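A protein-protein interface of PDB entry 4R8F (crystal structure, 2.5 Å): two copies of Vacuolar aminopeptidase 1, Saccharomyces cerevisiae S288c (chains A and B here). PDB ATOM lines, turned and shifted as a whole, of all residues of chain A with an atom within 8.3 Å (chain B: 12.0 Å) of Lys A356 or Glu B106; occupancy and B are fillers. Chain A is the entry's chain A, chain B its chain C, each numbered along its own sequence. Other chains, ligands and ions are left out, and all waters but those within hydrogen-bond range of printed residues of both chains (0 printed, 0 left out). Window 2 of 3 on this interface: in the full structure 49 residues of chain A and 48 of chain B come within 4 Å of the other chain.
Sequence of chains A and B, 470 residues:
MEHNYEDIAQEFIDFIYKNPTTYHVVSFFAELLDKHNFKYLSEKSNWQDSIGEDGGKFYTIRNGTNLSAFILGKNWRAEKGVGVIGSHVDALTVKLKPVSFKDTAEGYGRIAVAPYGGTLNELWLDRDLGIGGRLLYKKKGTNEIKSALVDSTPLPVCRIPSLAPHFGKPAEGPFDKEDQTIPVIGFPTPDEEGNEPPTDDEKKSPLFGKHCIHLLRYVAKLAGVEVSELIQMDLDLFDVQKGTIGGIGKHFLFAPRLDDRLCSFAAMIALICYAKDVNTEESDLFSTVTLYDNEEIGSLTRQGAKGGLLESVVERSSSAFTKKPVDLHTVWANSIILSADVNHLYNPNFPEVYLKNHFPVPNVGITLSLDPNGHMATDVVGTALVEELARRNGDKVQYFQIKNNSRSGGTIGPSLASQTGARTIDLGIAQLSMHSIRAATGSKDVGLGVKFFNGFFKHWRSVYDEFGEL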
ATOM      1  N   TYR A 346      14.285  25.415 -23.681  1.00  0.00           N
ATOM      2  CA  TYR A 346      13.623  26.249 -24.661  1.00  0.00           C
ATOM      3  C   TYR A 346      14.415  27.542 -24.798  1.00  0.00           C
ATOM      4  O   TYR A 346      14.578  28.281 -23.829  1.00  0.00           O
ATOM      5  CB  TYR A 346      12.196  26.560 -24.214  1.00  0.00           C
ATOM      6  CG  TYR A 346      11.361  27.263 -25.257  1.00  0.00           C
ATOM      7  CD1 TYR A 346      10.936  26.589 -26.398  1.00  0.00           C
ATOM      8  CD2 TYR A 346      10.982  28.595 -25.098  1.00  0.00           C
ATOM      9  CE1 TYR A 346      10.164  27.221 -27.358  1.00  0.00           C
ATOM     10  CE2 TYR A 346      10.210  29.236 -26.053  1.00  0.00           C
ATOM     11  CZ  TYR A 346       9.802  28.544 -27.180  1.00  0.00           C
ATOM     12  OH  TYR A 346       9.033  29.174 -28.127  1.00  0.00           O
ATOM     13  N   ASN A 347      14.940  27.780 -25.992  1.00  0.00           N
ATOM     14  CA  ASN A 347      15.540  29.052 -26.329  1.00  0.00           C
ATOM     15  C   ASN A 347      14.425  29.866 -26.976  1.00  0.00           C
ATOM     16  O   ASN A 347      13.961  29.523 -28.066  1.00  0.00           O
ATOM     17  CB  ASN A 347      16.717  28.853 -27.286  1.00  0.00           C
ATOM     18  CG  ASN A 347      17.562  30.106 -27.448  1.00  0.00           C
ATOM     19  OD1 ASN A 347      17.095  31.223 -27.223  1.00  0.00           O
ATOM     20  ND2 ASN A 347      18.816  29.921 -27.855  1.00  0.00           N
ATOM     21  N   PRO A 348      13.969  30.937 -26.297  1.00  0.00           N
ATOM     22  CA  PRO A 348      12.851  31.717 -26.831  1.00  0.00           C
ATOM     23  C   PRO A 348      13.197  32.456 -28.125  1.00  0.00           C
ATOM     24  O   PRO A 348      12.298  32.927 -28.819  1.00  0.00           O
ATOM     25  CB  PRO A 348      12.544  32.709 -25.703  1.00  0.00           C
ATOM     26  CG  PRO A 348      13.836  32.869 -24.982  1.00  0.00           C
ATOM     27  CD  PRO A 348      14.520  31.532 -25.064  1.00  0.00           C
ATOM     28  N   PRO A 351      12.142  29.489 -31.523  1.00  0.00           N
ATOM     29  CA  PRO A 351      10.963  28.634 -31.287  1.00  0.00           C
ATOM     30  C   PRO A 351      10.741  27.487 -32.284  1.00  0.00           C
ATOM     31  O   PRO A 351      10.167  26.462 -31.907  1.00  0.00           O
ATOM     32  CB  PRO A 351       9.778  29.616 -31.361  1.00  0.00           C
ATOM     33  CG  PRO A 351      10.333  30.935 -31.771  1.00  0.00           C
ATOM     34  CD  PRO A 351      11.796  30.919 -31.473  1.00  0.00           C
ATOM     35  N   GLU A 352      11.174  27.654 -33.533  1.00  0.00           N
ATOM     36  CA  GLU A 352      10.884  26.667 -34.583  1.00  0.00           C
ATOM     37  C   GLU A 352      11.641  25.340 -34.455  1.00  0.00           C
ATOM     38  O   GLU A 352      11.143  24.309 -34.910  1.00  0.00           O
ATOM     39  CB  GLU A 352      11.110  27.257 -35.985  1.00  0.00           C
ATOM     40  CG  GLU A 352       9.841  27.765 -36.661  1.00  0.00           C
ATOM     41  CD  GLU A 352       8.875  26.653 -37.054  1.00  0.00           C
ATOM     42  OE1 GLU A 352       9.198  25.459 -36.866  1.00  0.00           O
ATOM     43  OE2 GLU A 352       7.780  26.975 -37.560  1.00  0.00           O
ATOM     44  N   VAL A 353      12.825  25.351 -33.846  1.00  0.00           N
ATOM     45  CA  VAL A 353      13.588  24.108 -33.683  1.00  0.00           C
ATOM     46  C   VAL A 353      12.943  23.211 -32.616  1.00  0.00           C
ATOM     47  O   VAL A 353      13.113  21.992 -32.644  1.00  0.00           O
ATOM     48  CB  VAL A 353      15.090  24.347 -33.356  1.00  0.00           C
ATOM     49  CG1 VAL A 353      15.680  25.430 -34.252  1.00  0.00           C
ATOM     50  CG2 VAL A 353      15.300  24.701 -31.890  1.00  0.00           C
ATOM     51  N   TYR A 354      12.201  23.820 -31.689  1.00  0.00           N
ATOM     52  CA  TYR A 354      11.557  23.087 -30.597  1.00  0.00           C
ATOM     53  C   TYR A 354      10.171  22.593 -30.968  1.00  0.00           C
ATOM     54  O   TYR A 354       9.475  23.192 -31.789  1.00  0.00           O
ATOM     55  CB  TYR A 354      11.482  23.951 -29.335  1.00  0.00           C
ATOM     56  CG  TYR A 354      12.848  24.289 -28.813  1.00  0.00           C
ATOM     57  CD1 TYR A 354      13.521  25.411 -29.273  1.00  0.00           C
ATOM     58  CD2 TYR A 354      13.486  23.468 -27.891  1.00  0.00           C
ATOM     59  CE1 TYR A 354      14.792  25.721 -28.822  1.00  0.00           C
ATOM     60  CE2 TYR A 354      14.755  23.769 -27.427  1.00  0.00           C
ATOM     61  CZ  TYR A 354      15.406  24.897 -27.899  1.00  0.00           C
ATOM     62  OH  TYR A 354      16.667  25.209 -27.444  1.00  0.00           O
ATOM     63  N   LEU A 355       9.787  21.488 -30.339  1.00  0.00           N
ATOM     64  CA  LEU A 355       8.517  20.837 -30.592  1.00  0.00           C
ATOM     65  C   LEU A 355       7.545  21.161 -29.469  1.00  0.00           C
ATOM     66  O   LEU A 355       7.843  20.905 -28.305  1.00  0.00           O
ATOM     67  CB  LEU A 355       8.736  19.331 -30.677  1.00  0.00           C
ATOM     68  CG  LEU A 355       7.527  18.535 -31.162  1.00  0.00           C
ATOM     69  CD1 LEU A 355       7.961  17.508 -32.183  1.00  0.00           C
ATOM     70  CD2 LEU A 355       6.800  17.871 -30.010  1.00  0.00           C
ATOM     71  N   LYS A 356       6.379  21.705 -29.818  1.00  0.00           N
ATOM     72  CA  LYS A 356       5.416  22.153 -28.810  1.00  0.00           C
ATOM     73  C   LYS A 356       4.969  21.019 -27.884  1.00  0.00           C
ATOM     74  O   LYS A 356       4.660  19.919 -28.340  1.00  0.00           O
ATOM     75  CB  LYS A 356       4.196  22.825 -29.456  1.00  0.00           C
ATOM     76  CG  LYS A 356       3.309  23.576 -28.466  1.00  0.00           C
ATOM     77  CD  LYS A 356       3.975  24.846 -27.939  1.00  0.00           C
ATOM     78  CE  LYS A 356       3.574  25.171 -26.501  1.00  0.00           C
ATOM     79  NZ  LYS A 356       4.037  24.179 -25.488  1.00  0.00           N
ATOM     80  N   ASN A 357       4.980  21.308 -26.580  1.00  0.00           N
ATOM     81  CA  ASN A 357       4.585  20.377 -25.515  1.00  0.00           C
ATOM     82  C   ASN A 357       5.666  19.329 -25.270  1.00  0.00           C
ATOM     83  O   ASN A 357       5.424  18.302 -24.634  1.00  0.00           O
ATOM     84  CB  ASN A 357       3.227  19.712 -25.799  1.00  0.00           C
ATOM     85  CG  ASN A 357       2.096  20.719 -25.937  1.00  0.00           C
ATOM     86  OD1 ASN A 357       2.067  21.738 -25.243  1.00  0.00           O
ATOM     87  ND2 ASN A 357       1.150  20.433 -26.826  1.00  0.00           N
ATOM     88  N   HIS A 358       6.865  19.612 -25.771  1.00  0.00           N
ATOM     89  CA  HIS A 358       8.008  18.727 -25.645  1.00  0.00           C
ATOM     90  C   HIS A 358       9.286  19.569 -25.538  1.00  0.00           C
ATOM     91  O   HIS A 358      10.272  19.302 -26.230  1.00  0.00           O
ATOM     92  CB  HIS A 358       8.109  17.814 -26.866  1.00  0.00           C
ATOM     93  CG  HIS A 358       7.054  16.756 -26.947  1.00  0.00           C
ATOM     94  ND1 HIS A 358       7.287  15.449 -26.579  1.00  0.00           N
ATOM     95  CD2 HIS A 358       5.779  16.797 -27.400  1.00  0.00           C
ATOM     96  CE1 HIS A 358       6.198  14.734 -26.788  1.00  0.00           C
ATOM     97  NE2 HIS A 358       5.269  15.528 -27.287  1.00  0.00           N
ATOM     98  N   PHE A 359       9.252  20.607 -24.704  1.00  0.00           N
ATOM     99  CA  PHE A 359      10.454  21.387 -24.397  1.00  0.00           C
ATOM    100  C   PHE A 359      10.455  21.850 -22.938  1.00  0.00           C
ATOM    101  O   PHE A 359       9.441  22.333 -22.434  1.00  0.00           O
ATOM    102  CB  PHE A 359      10.632  22.577 -25.352  1.00  0.00           C
ATOM    103  CG  PHE A 359       9.424  23.460 -25.473  1.00  0.00           C
ATOM    104  CD1 PHE A 359       9.123  24.396 -24.492  1.00  0.00           C
ATOM    105  CD2 PHE A 359       8.603  23.381 -26.588  1.00  0.00           C
ATOM    106  CE1 PHE A 359       8.017  25.215 -24.609  1.00  0.00           C
ATOM    107  CE2 PHE A 359       7.499  24.204 -26.713  1.00  0.00           C
ATOM    108  CZ  PHE A 359       7.204  25.124 -25.724  1.00  0.00           C
ATOM    109  N   PRO A 360      11.597  21.686 -22.253  1.00  0.00           N
ATOM    110  CA  PRO A 360      11.706  22.057 -20.853  1.00  0.00           C
ATOM    111  C   PRO A 360      11.957  23.550 -20.647  1.00  0.00           C
ATOM    112  O   PRO A 360      12.490  24.225 -21.529  1.00  0.00           O
ATOM    113  CB  PRO A 360      12.916  21.250 -20.383  1.00  0.00           C
ATOM    114  CG  PRO A 360      13.780  21.172 -21.589  1.00  0.00           C
ATOM    115  CD  PRO A 360      12.834  21.054 -22.749  1.00  0.00           C
ATOM    116  N   VAL A 361      11.573  24.041 -19.477  1.00  0.00           N
ATOM    117  CA  VAL A 361      11.846  25.413 -19.068  1.00  0.00           C
ATOM    118  C   VAL A 361      12.727  25.353 -17.818  1.00  0.00           C
ATOM    119  O   VAL A 361      12.851  24.296 -17.207  1.00  0.00           O
ATOM    120  CB  VAL A 361      10.539  26.205 -18.804  1.00  0.00           C
ATOM    121  CG1 VAL A 361       9.645  26.185 -20.035  1.00  0.00           C
ATOM    122  CG2 VAL A 361       9.788  25.660 -17.600  1.00  0.00           C
ATOM    123  N   PRO A 362      13.346  26.478 -17.434  1.00  0.00           N
ATOM    124  CA  PRO A 362      14.252  26.421 -16.287  1.00  0.00           C
ATOM    125  C   PRO A 362      13.527  26.367 -14.938  1.00  0.00           C
ATOM    126  O   PRO A 362      12.349  26.717 -14.852  1.00  0.00           O
ATOM    127  CB  PRO A 362      15.071  27.716 -16.410  1.00  0.00           C
ATOM    128  CG  PRO A 362      14.408  28.554 -17.456  1.00  0.00           C
ATOM    129  CD  PRO A 362      13.185  27.850 -17.948  1.00  0.00           C
ATOM    130  N   TYR A 399       9.360  17.040 -20.413  1.00  0.00           N
ATOM    131  CA  TYR A 399       9.607  16.236 -21.594  1.00  0.00           C
ATOM    132  C   TYR A 399      10.445  16.996 -22.606  1.00  0.00           C
ATOM    133  O   TYR A 399      10.430  18.225 -22.656  1.00  0.00           O
ATOM    134  CB  TYR A 399       8.289  15.810 -22.239  1.00  0.00           C
ATOM    135  CG  TYR A 399       7.491  14.760 -21.483  1.00  0.00           C
ATOM    136  CD1 TYR A 399       8.000  14.104 -20.360  1.00  0.00           C
ATOM    137  CD2 TYR A 399       6.226  14.395 -21.929  1.00  0.00           C
ATOM    138  CE1 TYR A 399       7.260  13.139 -19.697  1.00  0.00           C
ATOM    139  CE2 TYR A 399       5.481  13.429 -21.273  1.00  0.00           C
ATOM    140  CZ  TYR A 399       6.000  12.804 -20.160  1.00  0.00           C
ATOM    141  OH  TYR A 399       5.249  11.848 -19.521  1.00  0.00           O
ATOM    142  N   GLN A 401      11.122  15.898 -26.675  1.00  0.00           N
ATOM    143  CA  GLN A 401      11.224  15.124 -27.901  1.00  0.00           C
ATOM    144  C   GLN A 401      11.879  16.021 -28.937  1.00  0.00           C
ATOM    145  O   GLN A 401      11.628  17.229 -28.976  1.00  0.00           O
ATOM    146  CB  GLN A 401       9.857  14.643 -28.389  1.00  0.00           C
ATOM    147  CG  GLN A 401       9.811  13.157 -28.737  1.00  0.00           C
ATOM    148  CD  GLN A 401       9.140  12.864 -30.068  1.00  0.00           C
ATOM    149  OE1 GLN A 401       9.259  13.635 -31.022  1.00  0.00           O
ATOM    150  NE2 GLN A 401       8.456  11.724 -30.151  1.00  0.00           N
ATOM    151  N   LYS B 102       8.901  43.590 -24.084  1.00  0.00           N
ATOM    152  CA  LYS B 102       8.783  42.340 -24.824  1.00  0.00           C
ATOM    153  C   LYS B 102       7.695  41.476 -24.209  1.00  0.00           C
ATOM    154  O   LYS B 102       7.641  41.310 -22.988  1.00  0.00           O
ATOM    155  CB  LYS B 102      10.114  41.587 -24.792  1.00  0.00           C
ATOM    156  CG  LYS B 102      11.028  41.902 -25.961  1.00  0.00           C
ATOM    157  CD  LYS B 102      10.749  40.995 -27.151  1.00  0.00           C
ATOM    158  CE  LYS B 102      10.772  41.761 -28.465  1.00  0.00           C
ATOM    159  NZ  LYS B 102      11.107  40.869 -29.609  1.00  0.00           N
ATOM    160  N   ASP B 103       6.830  40.930 -25.059  1.00  0.00           N
ATOM    161  CA  ASP B 103       5.801  39.995 -24.609  1.00  0.00           C
ATOM    162  C   ASP B 103       6.449  38.718 -24.084  1.00  0.00           C
ATOM    163  O   ASP B 103       7.507  38.306 -24.569  1.00  0.00           O
ATOM    164  CB  ASP B 103       4.810  39.663 -25.737  1.00  0.00           C
ATOM    165  CG  ASP B 103       3.472  40.366 -25.570  1.00  0.00           C
ATOM    166  OD1 ASP B 103       2.899  40.308 -24.459  1.00  0.00           O
ATOM    167  OD2 ASP B 103       2.983  40.963 -26.553  1.00  0.00           O
ATOM    168  N   THR B 104       5.811  38.102 -23.092  1.00  0.00           N
ATOM    169  CA  THR B 104       6.339  36.883 -22.480  1.00  0.00           C
ATOM    170  C   THR B 104       6.380  35.787 -23.553  1.00  0.00           C
ATOM    171  O   THR B 104       5.418  35.606 -24.306  1.00  0.00           O
ATOM    172  CB  THR B 104       5.529  36.463 -21.215  1.00  0.00           C
ATOM    173  OG1 THR B 104       6.427  36.217 -20.123  1.00  0.00           O
ATOM    174  CG2 THR B 104       4.654  35.217 -21.449  1.00  0.00           C
ATOM    175  N   ALA B 105       7.509  35.089 -23.637  1.00  0.00           N
ATOM    176  CA  ALA B 105       7.728  34.084 -24.671  1.00  0.00           C
ATOM    177  C   ALA B 105       7.926  32.717 -24.035  1.00  0.00           C
ATOM    178  O   ALA B 105       9.057  32.313 -23.742  1.00  0.00           O
ATOM    179  CB  ALA B 105       8.931  34.459 -25.524  1.00  0.00           C
ATOM    180  N   GLU B 106       6.814  32.017 -23.818  1.00  0.00           N
ATOM    181  CA  GLU B 106       6.822  30.673 -23.240  1.00  0.00           C
ATOM    182  C   GLU B 106       7.373  30.682 -21.800  1.00  0.00           C
ATOM    183  O   GLU B 106       8.010  29.720 -21.357  1.00  0.00           O
ATOM    184  CB  GLU B 106       7.615  29.722 -24.152  1.00  0.00           C
ATOM    185  CG  GLU B 106       6.990  28.351 -24.350  1.00  0.00           C
ATOM    186  CD  GLU B 106       5.652  28.393 -25.072  1.00  0.00           C
ATOM    187  OE1 GLU B 106       5.572  29.003 -26.161  1.00  0.00           O
ATOM    188  OE2 GLU B 106       4.680  27.802 -24.556  1.00  0.00           O
ATOM    189  N   GLY B 107       7.112  31.776 -21.081  1.00  0.00           N
ATOM    190  CA  GLY B 107       7.572  31.949 -19.701  1.00  0.00           C
ATOM    191  C   GLY B 107       8.741  32.909 -19.544  1.00  0.00           C
ATOM    192  O   GLY B 107       8.844  33.602 -18.529  1.00  0.00           O
ATOM    193  N   TYR B 108       9.625  32.949 -20.542  1.00  0.00           N
ATOM    194  CA  TYR B 108      10.808  33.810 -20.501  1.00  0.00           C
ATOM    195  C   TYR B 108      10.429  35.278 -20.594  1.00  0.00           C
ATOM    196  O   TYR B 108       9.489  35.643 -21.303  1.00  0.00           O
ATOM    197  CB  TYR B 108      11.759  33.490 -21.660  1.00  0.00           C
ATOM    198  CG  TYR B 108      12.502  32.182 -21.522  1.00  0.00           C
ATOM    199  CD1 TYR B 108      11.946  30.991 -21.981  1.00  0.00           C
ATOM    200  CD2 TYR B 108      13.767  32.137 -20.941  1.00  0.00           C
ATOM    201  CE1 TYR B 108      12.624  29.792 -21.859  1.00  0.00           C
ATOM    202  CE2 TYR B 108      14.453  30.941 -20.817  1.00  0.00           C
ATOM    203  CZ  TYR B 108      13.876  29.772 -21.275  1.00  0.00           C
ATOM    204  OH  TYR B 108      14.555  28.583 -21.154  1.00  0.00           O
ATOM    205  N   GLY B 109      11.173  36.116 -19.879  1.00  0.00           N
ATOM    206  CA  GLY B 109      11.094  37.554 -20.067  1.00  0.00           C
ATOM    207  C   GLY B 109      12.279  37.996 -20.897  1.00  0.00           C
ATOM    208  O   GLY B 109      13.397  37.501 -20.721  1.00  0.00           O
ATOM    209  N   ARG B 110      12.025  38.921 -21.812  1.00  0.00           N
ATOM    210  CA  ARG B 110      13.051  39.429 -22.703  1.00  0.00           C
ATOM    211  C   ARG B 110      12.933  40.940 -22.819  1.00  0.00           C
ATOM    212  O   ARG B 110      11.999  41.543 -22.284  1.00  0.00           O
ATOM    213  CB  ARG B 110      12.931  38.769 -24.078  1.00  0.00           C
ATOM    214  CG  ARG B 110      13.366  37.307 -24.093  1.00  0.00           C
ATOM    215  CD  ARG B 110      13.302  36.704 -25.487  1.00  0.00           C
ATOM    216  NE  ARG B 110      11.981  36.859 -26.096  1.00  0.00           N
ATOM    217  CZ  ARG B 110      11.680  36.504 -27.344  1.00  0.00           C
ATOM    218  NH1 ARG B 110      12.596  35.955 -28.137  1.00  0.00           N
ATOM    219  NH2 ARG B 110      10.448  36.697 -27.801  1.00  0.00           N
ATOM    220  N   ILE B 111      13.900  41.543 -23.499  1.00  0.00           N
ATOM    221  CA  ILE B 111      13.897  42.976 -23.745  1.00  0.00           C
ATOM    222  C   ILE B 111      14.323  43.231 -25.179  1.00  0.00           C
ATOM    223  O   ILE B 111      15.218  42.565 -25.703  1.00  0.00           O
ATOM    224  CB  ILE B 111      14.821  43.741 -22.770  1.00  0.00           C
ATOM    225  CG1 ILE B 111      16.135  42.973 -22.557  1.00  0.00           C
ATOM    226  CG2 ILE B 111      14.101  43.979 -21.448  1.00  0.00           C
ATOM    227  CD1 ILE B 111      17.190  43.716 -21.761  1.00  0.00           C
ATOM    228  N   PHE B 167      21.297  21.511 -34.007  1.00  0.00           N
ATOM    229  CA  PHE B 167      19.906  21.652 -34.441  1.00  0.00           C
ATOM    230  C   PHE B 167      19.824  21.851 -35.954  1.00  0.00           C
ATOM    231  O   PHE B 167      20.843  22.007 -36.629  1.00  0.00           O
ATOM    232  CB  PHE B 167      19.230  22.829 -33.723  1.00  0.00           C
ATOM    233  CG  PHE B 167      18.609  22.466 -32.399  1.00  0.00           C
ATOM    234  CD1 PHE B 167      17.507  21.619 -32.343  1.00  0.00           C
ATOM    235  CD2 PHE B 167      19.113  22.979 -31.207  1.00  0.00           C
ATOM    236  CE1 PHE B 167      16.928  21.282 -31.130  1.00  0.00           C
ATOM    237  CE2 PHE B 167      18.536  22.647 -29.991  1.00  0.00           C
ATOM    238  CZ  PHE B 167      17.442  21.798 -29.952  1.00  0.00           C
ATOM    239  N   THR B 181      17.497  38.237 -29.463  1.00  0.00           N
ATOM    240  CA  THR B 181      16.848  38.852 -28.310  1.00  0.00           C
ATOM    241  C   THR B 181      17.509  38.287 -27.043  1.00  0.00           C
ATOM    242  O   THR B 181      18.375  37.417 -27.129  1.00  0.00           O
ATOM    243  CB  THR B 181      15.324  38.606 -28.322  1.00  0.00           C
ATOM    244  OG1 THR B 181      14.854  38.591 -29.678  1.00  0.00           O
ATOM    245  CG2 THR B 181      14.571  39.696 -27.547  1.00  0.00           C
ATOM    246  N   ILE B 182      17.107  38.781 -25.876  1.00  0.00           N
ATOM    247  CA  ILE B 182      17.895  38.632 -24.664  1.00  0.00           C
ATOM    248  C   ILE B 182      17.019  38.238 -23.473  1.00  0.00           C
ATOM    249  O   ILE B 182      16.230  39.052 -22.997  1.00  0.00           O
ATOM    250  CB  ILE B 182      18.608  39.956 -24.325  1.00  0.00           C
ATOM    251  CG1 ILE B 182      19.243  40.582 -25.562  1.00  0.00           C
ATOM    252  CG2 ILE B 182      19.692  39.731 -23.303  1.00  0.00           C
ATOM    253  CD1 ILE B 182      18.272  41.389 -26.384  1.00  0.00           C
ATOM    254  N   PRO B 183      17.140  36.982 -22.999  1.00  0.00           N
ATOM    255  CA  PRO B 183      16.514  36.523 -21.750  1.00  0.00           C
ATOM    256  C   PRO B 183      16.945  37.290 -20.490  1.00  0.00           C
ATOM    257  O   PRO B 183      18.107  37.204 -20.084  1.00  0.00           O
ATOM    258  CB  PRO B 183      16.967  35.063 -21.655  1.00  0.00           C
ATOM    259  CG  PRO B 183      17.133  34.631 -23.068  1.00  0.00           C
ATOM    260  CD  PRO B 183      17.532  35.848 -23.858  1.00  0.00           C
ATOM    261  N   VAL B 184      16.008  38.026 -19.887  1.00  0.00           N
ATOM    262  CA  VAL B 184      16.262  38.753 -18.629  1.00  0.00           C
ATOM    263  C   VAL B 184      15.832  37.961 -17.392  1.00  0.00           C
ATOM    264  O   VAL B 184      16.535  37.964 -16.385  1.00  0.00           O
ATOM    265  CB  VAL B 184      15.596  40.162 -18.592  1.00  0.00           C
ATOM    266  CG1 VAL B 184      15.956  40.967 -19.828  1.00  0.00           C
ATOM    267  CG2 VAL B 184      14.083  40.084 -18.432  1.00  0.00           C
ATOM    268  N   ILE B 185      14.685  37.282 -17.482  1.00  0.00           N
ATOM    269  CA  ILE B 185      14.073  36.573 -16.337  1.00  0.00           C
ATOM    270  C   ILE B 185      13.683  35.141 -16.709  1.00  0.00           C
ATOM    271  O   ILE B 185      13.592  34.791 -17.889  1.00  0.00           O
ATOM    272  CB  ILE B 185      12.810  37.298 -15.782  1.00  0.00           C
ATOM    273  CG1 ILE B 185      11.870  37.725 -16.918  1.00  0.00           C
ATOM    274  CG2 ILE B 185      13.205  38.480 -14.908  1.00  0.00           C
ATOM    275  CD1 ILE B 185      10.787  38.721 -16.542  1.00  0.00           C
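Of the 16 printed residues of chain B, 4 touch a printed residue of chain A. Hydrophobic or aromatic side chains of chain B that line the printed part of chain A: Tyr B108 and Phe B167. Of the 17 printed residues of chain A, 6 touch a printed residue of chain B. Hydrophobic or aromatic side chains of chain A within 4 Å of the printed part of chain B: Tyr A346, Pro A348, Val A353, Phe A359 and Pro A362. Along chain A the printed residues that touch a printed residue of chain B span positions 346 to 362. Among the printed residues, 8 pairs touch across the chains.
Among the printed residues, pairs that only touch across the chains: Tyr A346 with Glu B106 (3.3 Å), Phe A359 with Glu B106 (3.3 Å), Pro A362 with Tyr B108 (3.6 Å), Pro A348 with Tyr B108 (3.8 Å) and Val A353 with Phe B167 (3.8 Å).
OH of Tyr B108 sits at hydrogen-bond distance from O of Tyr A346 (2.7 Å). The backbone carbonyl oxygen (O) of Pro A348 sits at hydrogen-bond distance from the guanidinium group (NH1) of Arg B110 (3.1 Å). NZ of Lys A356 is in salt-bridge range of OE2 of Glu B106.
No position is printed for both chains. Of the 8 pairs that touch across the chains among the printed residues, none has its exchanged pair printed and touching as well.
Lys A356 touches one residue of chain B. Glu B106 touches just these residues of chain A: Tyr A346 (3.3 Å), Lys A356 (3.5 Å) and Phe A359 (3.3 Å). No residue of chain B comes within 4 Å of Asn A357. No residue of chain B comes within 4 Å of His A358. Of chain B, only Glu B106 (3.3 Å) comes within 4 Å of Phe A359. Of the printed residues of chain B, Pro A348 touches Tyr B108 and Arg B110. Of the printed residues of chain B, Tyr A346 touches Glu B106 (3.3 Å) and Tyr B108 (2.7 Å). Gln A401 touches none of the printed residues of chain B. The nearest residue of chain B that does not touch Lys A356 is Ala B105 (9.1 Å).
N of Tyr A346 sits at hydrogen-bond distance from O of Pro A360 (3.0 Å). The side-chain amino group (NZ) of Lys A356 lies within hydrogen-bond range of the side-chain amide oxygen (OD1) of Asn A357, 3.1 Å away. The backbone carbonyl oxygen (O) of Tyr A399 sits at hydrogen-bond distance from the backbone NH (N) of Phe A359. The side-chain hydroxyl (OG1) of Thr B104 is in hydrogen-bond range of the backbone carbonyl oxygen (O) of Tyr B108 (3.3 Å).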
